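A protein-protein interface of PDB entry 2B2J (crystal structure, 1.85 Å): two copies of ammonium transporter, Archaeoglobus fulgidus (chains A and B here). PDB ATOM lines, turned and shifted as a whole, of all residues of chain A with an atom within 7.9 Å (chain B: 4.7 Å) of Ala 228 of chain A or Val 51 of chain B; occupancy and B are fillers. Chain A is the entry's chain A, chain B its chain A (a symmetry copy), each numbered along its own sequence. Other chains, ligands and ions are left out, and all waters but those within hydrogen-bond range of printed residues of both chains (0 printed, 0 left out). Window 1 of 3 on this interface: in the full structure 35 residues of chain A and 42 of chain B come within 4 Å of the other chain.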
ATOM      1  N   TRP A 198     -29.224 -20.075  23.225  1.00  0.00           N
ATOM      2  CA  TRP A 198     -27.948 -20.548  22.695  1.00  0.00           C
ATOM      3  C   TRP A 198     -26.845 -20.240  23.714  1.00  0.00           C
ATOM      4  O   TRP A 198     -26.049 -21.105  24.077  1.00  0.00           O
ATOM      5  CB  TRP A 198     -27.621 -19.857  21.375  1.00  0.00           C
ATOM      6  CG  TRP A 198     -26.476 -20.519  20.649  1.00  0.00           C
ATOM      7  CD1 TRP A 198     -25.286 -20.936  21.188  1.00  0.00           C
ATOM      8  CD2 TRP A 198     -26.416 -20.847  19.250  1.00  0.00           C
ATOM      9  NE1 TRP A 198     -24.496 -21.504  20.214  1.00  0.00           N
ATOM     10  CE2 TRP A 198     -25.165 -21.461  19.018  1.00  0.00           C
ATOM     11  CE3 TRP A 198     -27.300 -20.684  18.174  1.00  0.00           C
ATOM     12  CZ2 TRP A 198     -24.775 -21.911  17.747  1.00  0.00           C
ATOM     13  CZ3 TRP A 198     -26.908 -21.135  16.908  1.00  0.00           C
ATOM     14  CH2 TRP A 198     -25.659 -21.739  16.711  1.00  0.00           C
ATOM     15  N   VAL A 220     -18.872 -28.287  24.716  1.00  0.00           N
ATOM     16  CA  VAL A 220     -19.093 -26.958  24.158  1.00  0.00           C
ATOM     17  C   VAL A 220     -18.862 -26.932  22.651  1.00  0.00           C
ATOM     18  O   VAL A 220     -19.614 -26.298  21.903  1.00  0.00           O
ATOM     19  CB  VAL A 220     -18.182 -25.905  24.836  1.00  0.00           C
ATOM     20  CG1 VAL A 220     -18.235 -24.593  24.070  1.00  0.00           C
ATOM     21  CG2 VAL A 220     -18.623 -25.688  26.279  1.00  0.00           C
ATOM     22  N   VAL A 221     -17.822 -27.619  22.201  1.00  0.00           N
ATOM     23  CA  VAL A 221     -17.523 -27.652  20.775  1.00  0.00           C
ATOM     24  C   VAL A 221     -18.645 -28.346  19.992  1.00  0.00           C
ATOM     25  O   VAL A 221     -19.220 -27.777  19.061  1.00  0.00           O
ATOM     26  CB  VAL A 221     -16.191 -28.396  20.504  1.00  0.00           C
ATOM     27  CG1 VAL A 221     -15.938 -28.477  19.016  1.00  0.00           C
ATOM     28  CG2 VAL A 221     -15.045 -27.683  21.191  1.00  0.00           C
ATOM     29  N   VAL A 222     -18.968 -29.574  20.377  1.00  0.00           N
ATOM     30  CA  VAL A 222     -19.995 -30.304  19.669  1.00  0.00           C
ATOM     31  C   VAL A 222     -21.346 -29.644  19.787  1.00  0.00           C
ATOM     32  O   VAL A 222     -22.149 -29.709  18.858  1.00  0.00           O
ATOM     33  CB  VAL A 222     -20.083 -31.755  20.159  1.00  0.00           C
ATOM     34  CG1 VAL A 222     -18.789 -32.458  19.823  1.00  0.00           C
ATOM     35  CG2 VAL A 222     -20.350 -31.809  21.665  1.00  0.00           C
ATOM     36  N   THR A 223     -21.604 -28.998  20.918  1.00  0.00           N
ATOM     37  CA  THR A 223     -22.893 -28.354  21.090  1.00  0.00           C
ATOM     38  C   THR A 223     -23.079 -27.262  20.046  1.00  0.00           C
ATOM     39  O   THR A 223     -24.133 -27.155  19.423  1.00  0.00           O
ATOM     40  CB  THR A 223     -23.038 -27.772  22.496  1.00  0.00           C
ATOM     41  OG1 THR A 223     -22.923 -28.827  23.455  1.00  0.00           O
ATOM     42  CG2 THR A 223     -24.402 -27.136  22.664  1.00  0.00           C
ATOM     43  N   ASN A 224     -22.048 -26.453  19.842  1.00  0.00           N
ATOM     44  CA  ASN A 224     -22.125 -25.382  18.854  1.00  0.00           C
ATOM     45  C   ASN A 224     -22.215 -25.955  17.447  1.00  0.00           C
ATOM     46  O   ASN A 224     -22.885 -25.397  16.572  1.00  0.00           O
ATOM     47  CB  ASN A 224     -20.902 -24.483  18.974  1.00  0.00           C
ATOM     48  CG  ASN A 224     -21.025 -23.502  20.116  1.00  0.00           C
ATOM     49  OD1 ASN A 224     -21.685 -22.476  19.986  1.00  0.00           O
ATOM     50  ND2 ASN A 224     -20.407 -23.818  21.250  1.00  0.00           N
ATOM     51  N   THR A 225     -21.540 -27.085  17.249  1.00  0.00           N
ATOM     52  CA  THR A 225     -21.514 -27.765  15.965  1.00  0.00           C
ATOM     53  C   THR A 225     -22.888 -28.298  15.582  1.00  0.00           C
ATOM     54  O   THR A 225     -23.430 -27.949  14.528  1.00  0.00           O
ATOM     55  CB  THR A 225     -20.521 -28.933  15.994  1.00  0.00           C
ATOM     56  OG1 THR A 225     -19.196 -28.423  16.174  1.00  0.00           O
ATOM     57  CG2 THR A 225     -20.572 -29.709  14.696  1.00  0.00           C
ATOM     58  N   SER A 226     -23.451 -29.156  16.426  1.00  0.00           N
ATOM     59  CA  SER A 226     -24.766 -29.703  16.139  1.00  0.00           C
ATOM     60  C   SER A 226     -25.760 -28.568  15.881  1.00  0.00           C
ATOM     61  O   SER A 226     -26.574 -28.638  14.960  1.00  0.00           O
ATOM     62  CB  SER A 226     -25.247 -30.549  17.308  1.00  0.00           C
ATOM     63  OG  SER A 226     -26.552 -31.039  17.063  1.00  0.00           O
ATOM     64  N   ALA A 227     -25.679 -27.511  16.682  1.00  0.00           N
ATOM     65  CA  ALA A 227     -26.579 -26.371  16.538  1.00  0.00           C
ATOM     66  C   ALA A 227     -26.461 -25.671  15.178  1.00  0.00           C
ATOM     67  O   ALA A 227     -27.473 -25.359  14.540  1.00  0.00           O
ATOM     68  CB  ALA A 227     -26.327 -25.374  17.661  1.00  0.00           C
ATOM     69  N   ALA A 228     -25.231 -25.421  14.734  1.00  0.00           N
ATOM     70  CA  ALA A 228     -25.001 -24.747  13.455  1.00  0.00           C
ATOM     71  C   ALA A 228     -25.476 -25.602  12.285  1.00  0.00           C
ATOM     72  O   ALA A 228     -26.105 -25.101  11.343  1.00  0.00           O
ATOM     73  CB  ALA A 228     -23.519 -24.417  13.298  1.00  0.00           C
ATOM     74  N   VAL A 229     -25.166 -26.894  12.350  1.00  0.00           N
ATOM     75  CA  VAL A 229     -25.562 -27.824  11.305  1.00  0.00           C
ATOM     76  C   VAL A 229     -27.081 -27.861  11.145  1.00  0.00           C
ATOM     77  O   VAL A 229     -27.600 -27.648  10.043  1.00  0.00           O
ATOM     78  CB  VAL A 229     -25.035 -29.247  11.608  1.00  0.00           C
ATOM     79  CG1 VAL A 229     -25.607 -30.250  10.626  1.00  0.00           C
ATOM     80  CG2 VAL A 229     -23.525 -29.258  11.526  1.00  0.00           C
ATOM     81  N   ALA A 230     -27.792 -28.119  12.244  1.00  0.00           N
ATOM     82  CA  ALA A 230     -29.260 -28.189  12.219  1.00  0.00           C
ATOM     83  C   ALA A 230     -29.902 -26.851  11.835  1.00  0.00           C
ATOM     84  O   ALA A 230     -31.001 -26.822  11.277  1.00  0.00           O
ATOM     85  CB  ALA A 230     -29.792 -28.660  13.583  1.00  0.00           C
ATOM     86  N   GLY A 231     -29.223 -25.748  12.151  1.00  0.00           N
ATOM     87  CA  GLY A 231     -29.750 -24.443  11.803  1.00  0.00           C
ATOM     88  C   GLY A 231     -29.604 -24.257  10.307  1.00  0.00           C
ATOM     89  O   GLY A 231     -30.463 -23.676   9.639  1.00  0.00           O
ATOM     90  N   PHE A 232     -28.500 -24.767   9.780  1.00  0.00           N
ATOM     91  CA  PHE A 232     -28.218 -24.684   8.354  1.00  0.00           C
ATOM     92  C   PHE A 232     -29.249 -25.519   7.578  1.00  0.00           C
ATOM     93  O   PHE A 232     -29.764 -25.104   6.533  1.00  0.00           O
ATOM     94  CB  PHE A 232     -26.806 -25.205   8.093  1.00  0.00           C
ATOM     95  CG  PHE A 232     -26.376 -25.086   6.667  1.00  0.00           C
ATOM     96  CD1 PHE A 232     -26.000 -23.857   6.142  1.00  0.00           C
ATOM     97  CD2 PHE A 232     -26.352 -26.206   5.840  1.00  0.00           C
ATOM     98  CE1 PHE A 232     -25.603 -23.747   4.812  1.00  0.00           C
ATOM     99  CE2 PHE A 232     -25.958 -26.104   4.510  1.00  0.00           C
ATOM    100  CZ  PHE A 232     -25.583 -24.876   3.997  1.00  0.00           C
ATOM    101  N   VAL A 233     -29.550 -26.701   8.101  1.00  0.00           N
ATOM    102  CA  VAL A 233     -30.521 -27.581   7.469  1.00  0.00           C
ATOM    103  C   VAL A 233     -31.873 -26.888   7.329  1.00  0.00           C
ATOM    104  O   VAL A 233     -32.440 -26.848   6.243  1.00  0.00           O
ATOM    105  CB  VAL A 233     -30.691 -28.879   8.283  1.00  0.00           C
ATOM    106  CG1 VAL A 233     -31.801 -29.746   7.688  1.00  0.00           C
ATOM    107  CG2 VAL A 233     -29.372 -29.631   8.310  1.00  0.00           C
ATOM    108  N   TRP A 234     -32.397 -26.342   8.420  1.00  0.00           N
ATOM    109  CA  TRP A 234     -33.684 -25.668   8.332  1.00  0.00           C
ATOM    110  C   TRP A 234     -33.580 -24.454   7.439  1.00  0.00           C
ATOM    111  O   TRP A 234     -34.580 -24.003   6.897  1.00  0.00           O
ATOM    112  CB  TRP A 234     -34.195 -25.249   9.709  1.00  0.00           C
ATOM    113  CG  TRP A 234     -34.777 -26.380  10.469  1.00  0.00           C
ATOM    114  CD1 TRP A 234     -34.178 -27.572  10.732  1.00  0.00           C
ATOM    115  CD2 TRP A 234     -36.070 -26.430  11.091  1.00  0.00           C
ATOM    116  NE1 TRP A 234     -35.010 -28.367  11.481  1.00  0.00           N
ATOM    117  CE2 TRP A 234     -36.179 -27.694  11.718  1.00  0.00           C
ATOM    118  CE3 TRP A 234     -37.144 -25.535  11.181  1.00  0.00           C
ATOM    119  CZ2 TRP A 234     -37.327 -28.089  12.433  1.00  0.00           C
ATOM    120  CZ3 TRP A 234     -38.289 -25.925  11.891  1.00  0.00           C
ATOM    121  CH2 TRP A 234     -38.368 -27.195  12.507  1.00  0.00           C
ATOM    122  N   MET A 235     -32.376 -23.917   7.283  1.00  0.00           N
ATOM    123  CA  MET A 235     -32.223 -22.757   6.419  1.00  0.00           C
ATOM    124  C   MET A 235     -32.365 -23.216   4.973  1.00  0.00           C
ATOM    125  O   MET A 235     -33.016 -22.542   4.171  1.00  0.00           O
ATOM    126  CB  MET A 235     -30.862 -22.083   6.617  1.00  0.00           C
ATOM    127  CG  MET A 235     -30.769 -20.684   5.997  1.00  0.00           C
ATOM    128  SD  MET A 235     -29.120 -19.966   6.111  1.00  0.00           S
ATOM    129  CE  MET A 235     -28.708 -20.345   7.814  1.00  0.00           C
ATOM    130  N   ILE A 249     -34.884 -20.898  11.076  1.00  0.00           N
ATOM    131  CA  ILE A 249     -33.458 -20.997  11.364  1.00  0.00           C
ATOM    132  C   ILE A 249     -33.135 -21.292  12.833  1.00  0.00           C
ATOM    133  O   ILE A 249     -32.340 -22.181  13.126  1.00  0.00           O
ATOM    134  CB  ILE A 249     -32.733 -19.709  10.912  1.00  0.00           C
ATOM    135  CG1 ILE A 249     -32.909 -19.543   9.397  1.00  0.00           C
ATOM    136  CG2 ILE A 249     -31.257 -19.769  11.279  1.00  0.00           C
ATOM    137  CD1 ILE A 249     -32.393 -18.243   8.855  1.00  0.00           C
ATOM    138  N   GLY A 252     -34.322 -24.600  13.964  1.00  0.00           N
ATOM    139  CA  GLY A 252     -33.418 -25.617  13.457  1.00  0.00           C
ATOM    140  C   GLY A 252     -32.240 -25.788  14.399  1.00  0.00           C
ATOM    141  O   GLY A 252     -31.850 -26.911  14.746  1.00  0.00           O
ATOM    142  N   ALA A 253     -31.673 -24.665  14.829  1.00  0.00           N
ATOM    143  CA  ALA A 253     -30.536 -24.688  15.749  1.00  0.00           C
ATOM    144  C   ALA A 253     -30.922 -25.335  17.079  1.00  0.00           C
ATOM    145  O   ALA A 253     -30.153 -26.107  17.661  1.00  0.00           O
ATOM    146  CB  ALA A 253     -30.037 -23.273  15.988  1.00  0.00           C
ATOM    147  N   ILE A 254     -32.116 -25.012  17.559  1.00  0.00           N
ATOM    148  CA  ILE A 254     -32.576 -25.569  18.812  1.00  0.00           C
ATOM    149  C   ILE A 254     -32.718 -27.078  18.693  1.00  0.00           C
ATOM    150  O   ILE A 254     -32.370 -27.811  19.616  1.00  0.00           O
ATOM    151  CB  ILE A 254     -33.888 -24.903  19.248  1.00  0.00           C
ATOM    152  CG1 ILE A 254     -33.598 -23.428  19.576  1.00  0.00           C
ATOM    153  CG2 ILE A 254     -34.476 -25.626  20.457  1.00  0.00           C
ATOM    154  CD1 ILE A 254     -34.768 -22.640  20.078  1.00  0.00           C
ATOM    155  N   GLY A 256     -30.944 -28.953  16.873  1.00  0.00           N
ATOM    156  CA  GLY A 256     -29.583 -29.442  16.942  1.00  0.00           C
ATOM    157  C   GLY A 256     -29.071 -29.415  18.364  1.00  0.00           C
ATOM    158  O   GLY A 256     -28.308 -30.294  18.776  1.00  0.00           O
ATOM    159  N   LEU A 257     -29.485 -28.410  19.129  1.00  0.00           N
ATOM    160  CA  LEU A 257     -29.042 -28.292  20.516  1.00  0.00           C
ATOM    161  C   LEU A 257     -29.628 -29.383  21.399  1.00  0.00           C
ATOM    162  O   LEU A 257     -28.933 -29.940  22.255  1.00  0.00           O
ATOM    163  CB  LEU A 257     -29.418 -26.921  21.074  1.00  0.00           C
ATOM    164  CG  LEU A 257     -28.560 -25.767  20.559  1.00  0.00           C
ATOM    165  CD1 LEU A 257     -29.174 -24.439  20.980  1.00  0.00           C
ATOM    166  CD2 LEU A 257     -27.132 -25.908  21.094  1.00  0.00           C
ATOM    167  N   VAL A 269     -16.450 -34.366  16.900  1.00  0.00           N
ATOM    168  CA  VAL A 269     -16.989 -33.362  15.989  1.00  0.00           C
ATOM    169  C   VAL A 269     -17.740 -33.934  14.788  1.00  0.00           C
ATOM    170  O   VAL A 269     -18.812 -33.443  14.425  1.00  0.00           O
ATOM    171  CB  VAL A 269     -15.867 -32.423  15.480  1.00  0.00           C
ATOM    172  CG1 VAL A 269     -14.976 -33.147  14.484  1.00  0.00           C
ATOM    173  CG2 VAL A 269     -16.475 -31.188  14.853  1.00  0.00           C
ATOM    174  N   ALA A 272     -20.989 -35.078  15.842  1.00  0.00           N
ATOM    175  CA  ALA A 272     -21.823 -33.919  16.125  1.00  0.00           C
ATOM    176  C   ALA A 272     -22.428 -33.435  14.823  1.00  0.00           C
ATOM    177  O   ALA A 272     -23.548 -32.942  14.796  1.00  0.00           O
ATOM    178  CB  ALA A 272     -20.992 -32.820  16.757  1.00  0.00           C
ATOM    179  N   GLY A 276     -26.474 -33.442  14.226  1.00  0.00           N
ATOM    180  CA  GLY A 276     -27.162 -32.212  13.866  1.00  0.00           C
ATOM    181  C   GLY A 276     -27.851 -32.303  12.514  1.00  0.00           C
ATOM    182  O   GLY A 276     -28.988 -31.861  12.341  1.00  0.00           O
ATOM    183  N   LEU A 277     -27.156 -32.876  11.544  1.00  0.00           N
ATOM    184  CA  LEU A 277     -27.706 -33.026  10.214  1.00  0.00           C
ATOM    185  C   LEU A 277     -29.041 -33.779  10.285  1.00  0.00           C
ATOM    186  O   LEU A 277     -30.062 -33.313   9.783  1.00  0.00           O
ATOM    187  CB  LEU A 277     -26.705 -33.785   9.355  1.00  0.00           C
ATOM    188  CG  LEU A 277     -26.542 -33.276   7.930  1.00  0.00           C
ATOM    189  CD1 LEU A 277     -25.328 -33.944   7.284  1.00  0.00           C
ATOM    190  CD2 LEU A 277     -27.814 -33.557   7.150  1.00  0.00           C
ATOM    191  N   LEU B  47     -23.383 -16.348  12.626  1.00  0.00           N
ATOM    192  CA  LEU B  47     -22.919 -17.314  13.600  1.00  0.00           C
ATOM    193  C   LEU B  47     -22.862 -18.693  12.980  1.00  0.00           C
ATOM    194  O   LEU B  47     -21.825 -19.352  13.012  1.00  0.00           O
ATOM    195  CB  LEU B  47     -23.836 -17.349  14.818  1.00  0.00           C
ATOM    196  CG  LEU B  47     -23.367 -18.320  15.908  1.00  0.00           C
ATOM    197  CD1 LEU B  47     -22.025 -17.866  16.473  1.00  0.00           C
ATOM    198  CD2 LEU B  47     -24.400 -18.393  17.004  1.00  0.00           C
ATOM    199  N   ILE B  48     -23.985 -19.123  12.414  1.00  0.00           N
ATOM    200  CA  ILE B  48     -24.085 -20.440  11.798  1.00  0.00           C
ATOM    201  C   ILE B  48     -23.056 -20.709  10.712  1.00  0.00           C
ATOM    202  O   ILE B  48     -22.356 -21.720  10.760  1.00  0.00           O
ATOM    203  CB  ILE B  48     -25.483 -20.664  11.209  1.00  0.00           C
ATOM    204  CG1 ILE B  48     -26.507 -20.685  12.343  1.00  0.00           C
ATOM    205  CG2 ILE B  48     -25.526 -21.974  10.425  1.00  0.00           C
ATOM    206  CD1 ILE B  48     -27.934 -20.607  11.862  1.00  0.00           C
ATOM    207  N   ILE B  49     -22.952 -19.816   9.735  1.00  0.00           N
ATOM    208  CA  ILE B  49     -21.991 -20.045   8.671  1.00  0.00           C
ATOM    209  C   ILE B  49     -20.546 -20.027   9.189  1.00  0.00           C
ATOM    210  O   ILE B  49     -19.682 -20.745   8.678  1.00  0.00           O
ATOM    211  CB  ILE B  49     -22.191 -19.037   7.503  1.00  0.00           C
ATOM    212  CG1 ILE B  49     -22.113 -17.595   8.005  1.00  0.00           C
ATOM    213  CG2 ILE B  49     -23.565 -19.278   6.859  1.00  0.00           C
ATOM    214  CD1 ILE B  49     -22.324 -16.530   6.902  1.00  0.00           C
ATOM    215  N   THR B  50     -20.284 -19.248  10.227  1.00  0.00           N
ATOM    216  CA  THR B  50     -18.938 -19.185  10.769  1.00  0.00           C
ATOM    217  C   THR B  50     -18.543 -20.473  11.466  1.00  0.00           C
ATOM    218  O   THR B  50     -17.460 -21.015  11.245  1.00  0.00           O
ATOM    219  CB  THR B  50     -18.810 -18.026  11.747  1.00  0.00           C
ATOM    220  OG1 THR B  50     -18.979 -16.801  11.032  1.00  0.00           O
ATOM    221  CG2 THR B  50     -17.446 -18.017  12.402  1.00  0.00           C
ATOM    222  N   VAL B  51     -19.417 -20.970  12.323  1.00  0.00           N
ATOM    223  CA  VAL B  51     -19.099 -22.197  13.016  1.00  0.00           C
ATOM    224  C   VAL B  51     -18.725 -23.264  11.994  1.00  0.00           C
ATOM    225  O   VAL B  51     -17.689 -23.915  12.109  1.00  0.00           O
ATOM    226  CB  VAL B  51     -20.288 -22.681  13.857  1.00  0.00           C
ATOM    227  CG1 VAL B  51     -19.994 -24.045  14.441  1.00  0.00           C
ATOM    228  CG2 VAL B  51     -20.558 -21.697  14.966  1.00  0.00           C
ATOM    229  N   LEU B  52     -19.557 -23.418  10.977  1.00  0.00           N
ATOM    230  CA  LEU B  52     -19.303 -24.423   9.959  1.00  0.00           C
ATOM    231  C   LEU B  52     -17.991 -24.207   9.204  1.00  0.00           C
ATOM    232  O   LEU B  52     -17.220 -25.144   9.031  1.00  0.00           O
ATOM    233  CB  LEU B  52     -20.475 -24.484   8.976  1.00  0.00           C
ATOM    234  CG  LEU B  52     -21.858 -24.718   9.590  1.00  0.00           C
ATOM    235  CD1 LEU B  52     -22.919 -24.683   8.516  1.00  0.00           C
ATOM    236  CD2 LEU B  52     -21.875 -26.039  10.301  1.00  0.00           C
ATOM    237  N   LEU B  53     -17.720 -22.991   8.756  1.00  0.00           N
ATOM    238  CA  LEU B  53     -16.480 -22.762   8.025  1.00  0.00           C
ATOM    239  C   LEU B  53     -15.259 -22.903   8.918  1.00  0.00           C
ATOM    240  O   LEU B  53     -14.239 -23.453   8.511  1.00  0.00           O
ATOM    241  CB  LEU B  53     -16.490 -21.375   7.383  1.00  0.00           C
ATOM    242  CG  LEU B  53     -17.576 -21.230   6.316  1.00  0.00           C
ATOM    243  CD1 LEU B  53     -17.503 -19.863   5.658  1.00  0.00           C
ATOM    244  CD2 LEU B  53     -17.389 -22.337   5.281  1.00  0.00           C
ATOM    245  N   TRP B  54     -15.376 -22.411  10.144  1.00  0.00           N
ATOM    246  CA  TRP B  54     -14.275 -22.457  11.091  1.00  0.00           C
ATOM    247  C   TRP B  54     -13.769 -23.874  11.330  1.00  0.00           C
ATOM    248  O   TRP B  54     -12.572 -24.146  11.265  1.00  0.00           O
ATOM    249  CB  TRP B  54     -14.713 -21.849  12.413  1.00  0.00           C
ATOM    250  CG  TRP B  54     -13.575 -21.597  13.329  1.00  0.00           C
ATOM    251  CD1 TRP B  54     -13.270 -22.275  14.478  1.00  0.00           C
ATOM    252  CD2 TRP B  54     -12.600 -20.558  13.202  1.00  0.00           C
ATOM    253  NE1 TRP B  54     -12.168 -21.711  15.080  1.00  0.00           N
ATOM    254  CE2 TRP B  54     -11.737 -20.655  14.317  1.00  0.00           C
ATOM    255  CE3 TRP B  54     -12.374 -19.547  12.256  1.00  0.00           C
ATOM    256  CZ2 TRP B  54     -10.662 -19.775  14.512  1.00  0.00           C
ATOM    257  CZ3 TRP B  54     -11.307 -18.672  12.450  1.00  0.00           C
ATOM    258  CH2 TRP B  54     -10.465 -18.792  13.572  1.00  0.00           C
ATOM    259  N   ILE B  55     -14.693 -24.772  11.632  1.00  0.00           N
ATOM    260  CA  ILE B  55     -14.357 -26.162  11.883  1.00  0.00           C
ATOM    261  C   ILE B  55     -13.842 -26.778  10.599  1.00  0.00           C
ATOM    262  O   ILE B  55     -12.758 -27.354  10.552  1.00  0.00           O
ATOM    263  CB  ILE B  55     -15.591 -26.974  12.268  1.00  0.00           C
ATOM    264  CG1 ILE B  55     -16.299 -26.345  13.455  1.00  0.00           C
ATOM    265  CG2 ILE B  55     -15.178 -28.383  12.597  1.00  0.00           C
ATOM    266  CD1 ILE B  55     -17.631 -27.012  13.750  1.00  0.00           C
ATOM    267  N   MET B  94     -13.300 -18.971  17.248  1.00  0.00           N
ATOM    268  CA  MET B  94     -14.404 -19.127  16.319  1.00  0.00           C
ATOM    269  C   MET B  94     -15.368 -17.971  16.534  1.00  0.00           C
ATOM    270  O   MET B  94     -15.811 -17.333  15.576  1.00  0.00           O
ATOM    271  CB  MET B  94     -15.123 -20.448  16.581  1.00  0.00           C
ATOM    272  CG  MET B  94     -16.365 -20.659  15.744  1.00  0.00           C
ATOM    273  SD  MET B  94     -17.275 -22.073  16.347  1.00  0.00           S
ATOM    274  CE  MET B  94     -16.443 -23.368  15.474  1.00  0.00           C
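NE1 of Trp 198 of chain A is in hydrogen-bond range of OD1 of Asn 224 of chain A (3.0 Å).
The backbone carbonyl oxygen (O) of Val 221 of chain A sits at hydrogen-bond distance from the side-chain hydroxyl (OG1) of Thr 225 of chain A (3.0 Å).
The side-chain amide nitrogen (ND2) of Asn 224 of chain A sits at hydrogen-bond distance from the backbone carbonyl oxygen (O) of Val 220 of chain A (2.7 Å).
No position is printed for both chains.
Of the 10 pairs that touch across the chains among the printed residues, none has its exchanged pair printed and touching as well.
Of the printed residues of chain B, Ala 228 of chain A touches Ile 48 (3.3 Å), Val 51 (3.7 Å) and Leu 52 (3.8 Å).
Of chain A, only Asn 224 and Ala 228 come within 4 Å of Val 51 of chain B.
Printed residues of chain A within 4 Å of Ile 48 of chain B: Ala 228 (3.3 Å) and Ile 249 (3.5 Å).
Of the printed residues of chain A, Ile 55 of chain B touches Thr 225 (3.2 Å) and Val 269 (3.8 Å).
Of the printed residues of chain A, Leu 52 of chain B touches Ala 228 (3.8 Å), Val 229 (3.8 Å) and Phe 232 (3.9 Å).
Of the printed residues of chain B, Asn 224 of chain A touches Val 51 (3.8 Å).
The nearest printed residue of chain B that does not touch Val 269 of chain A is Met 94 of chain B (7.8 Å).
CH2 of Trp 198 of chain A touches CD2 of Leu 47 of chain B, at 3.6 Å.
Asn 224 of chain A touches Val 51 of chain B.
Ile 55 of chain B touches Thr 225 of chain A (CD1 to OG1, 3.2 Å).
Ile 48 of chain B touches Ala 228 of chain A (CG2 to O, 3.3 Å).
Val 51 of chain B touches Ala 228 of chain A.
CD2 of Leu 52 of chain B touches CB of Ala 228 of chain A (3.8 Å).
CD2 of Leu 52 of chain B touches CG2 of Val 229 of chain A (3.8 Å).
Phe 232 of chain A touches Leu 52 of chain B.
Ile 249 of chain A touches Ile 48 of chain B.
CG2 of Val 269 of chain A touches CG2 of Ile 55 of chain B (3.8 Å).
Hydrophobic or aromatic side chains of chain A that line the printed part of chain B: Trp 198, Ala 228, Val 229, Phe 232, Ile 249 and Val 269.
Of the 10 printed residues of chain B, 5 touch a printed residue of chain A.
Printed residues of chain B that touch a printed residue of chain A: Leu 47, Ile 48, Val 51, Leu 52 and Ile 55.
Among the printed residues, 10 pairs touch across the chains.
Among the printed residues, no Asp or Glu carboxylate lies within 4 Å of a Lys or Arg side-chain nitrogen of the other chain.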
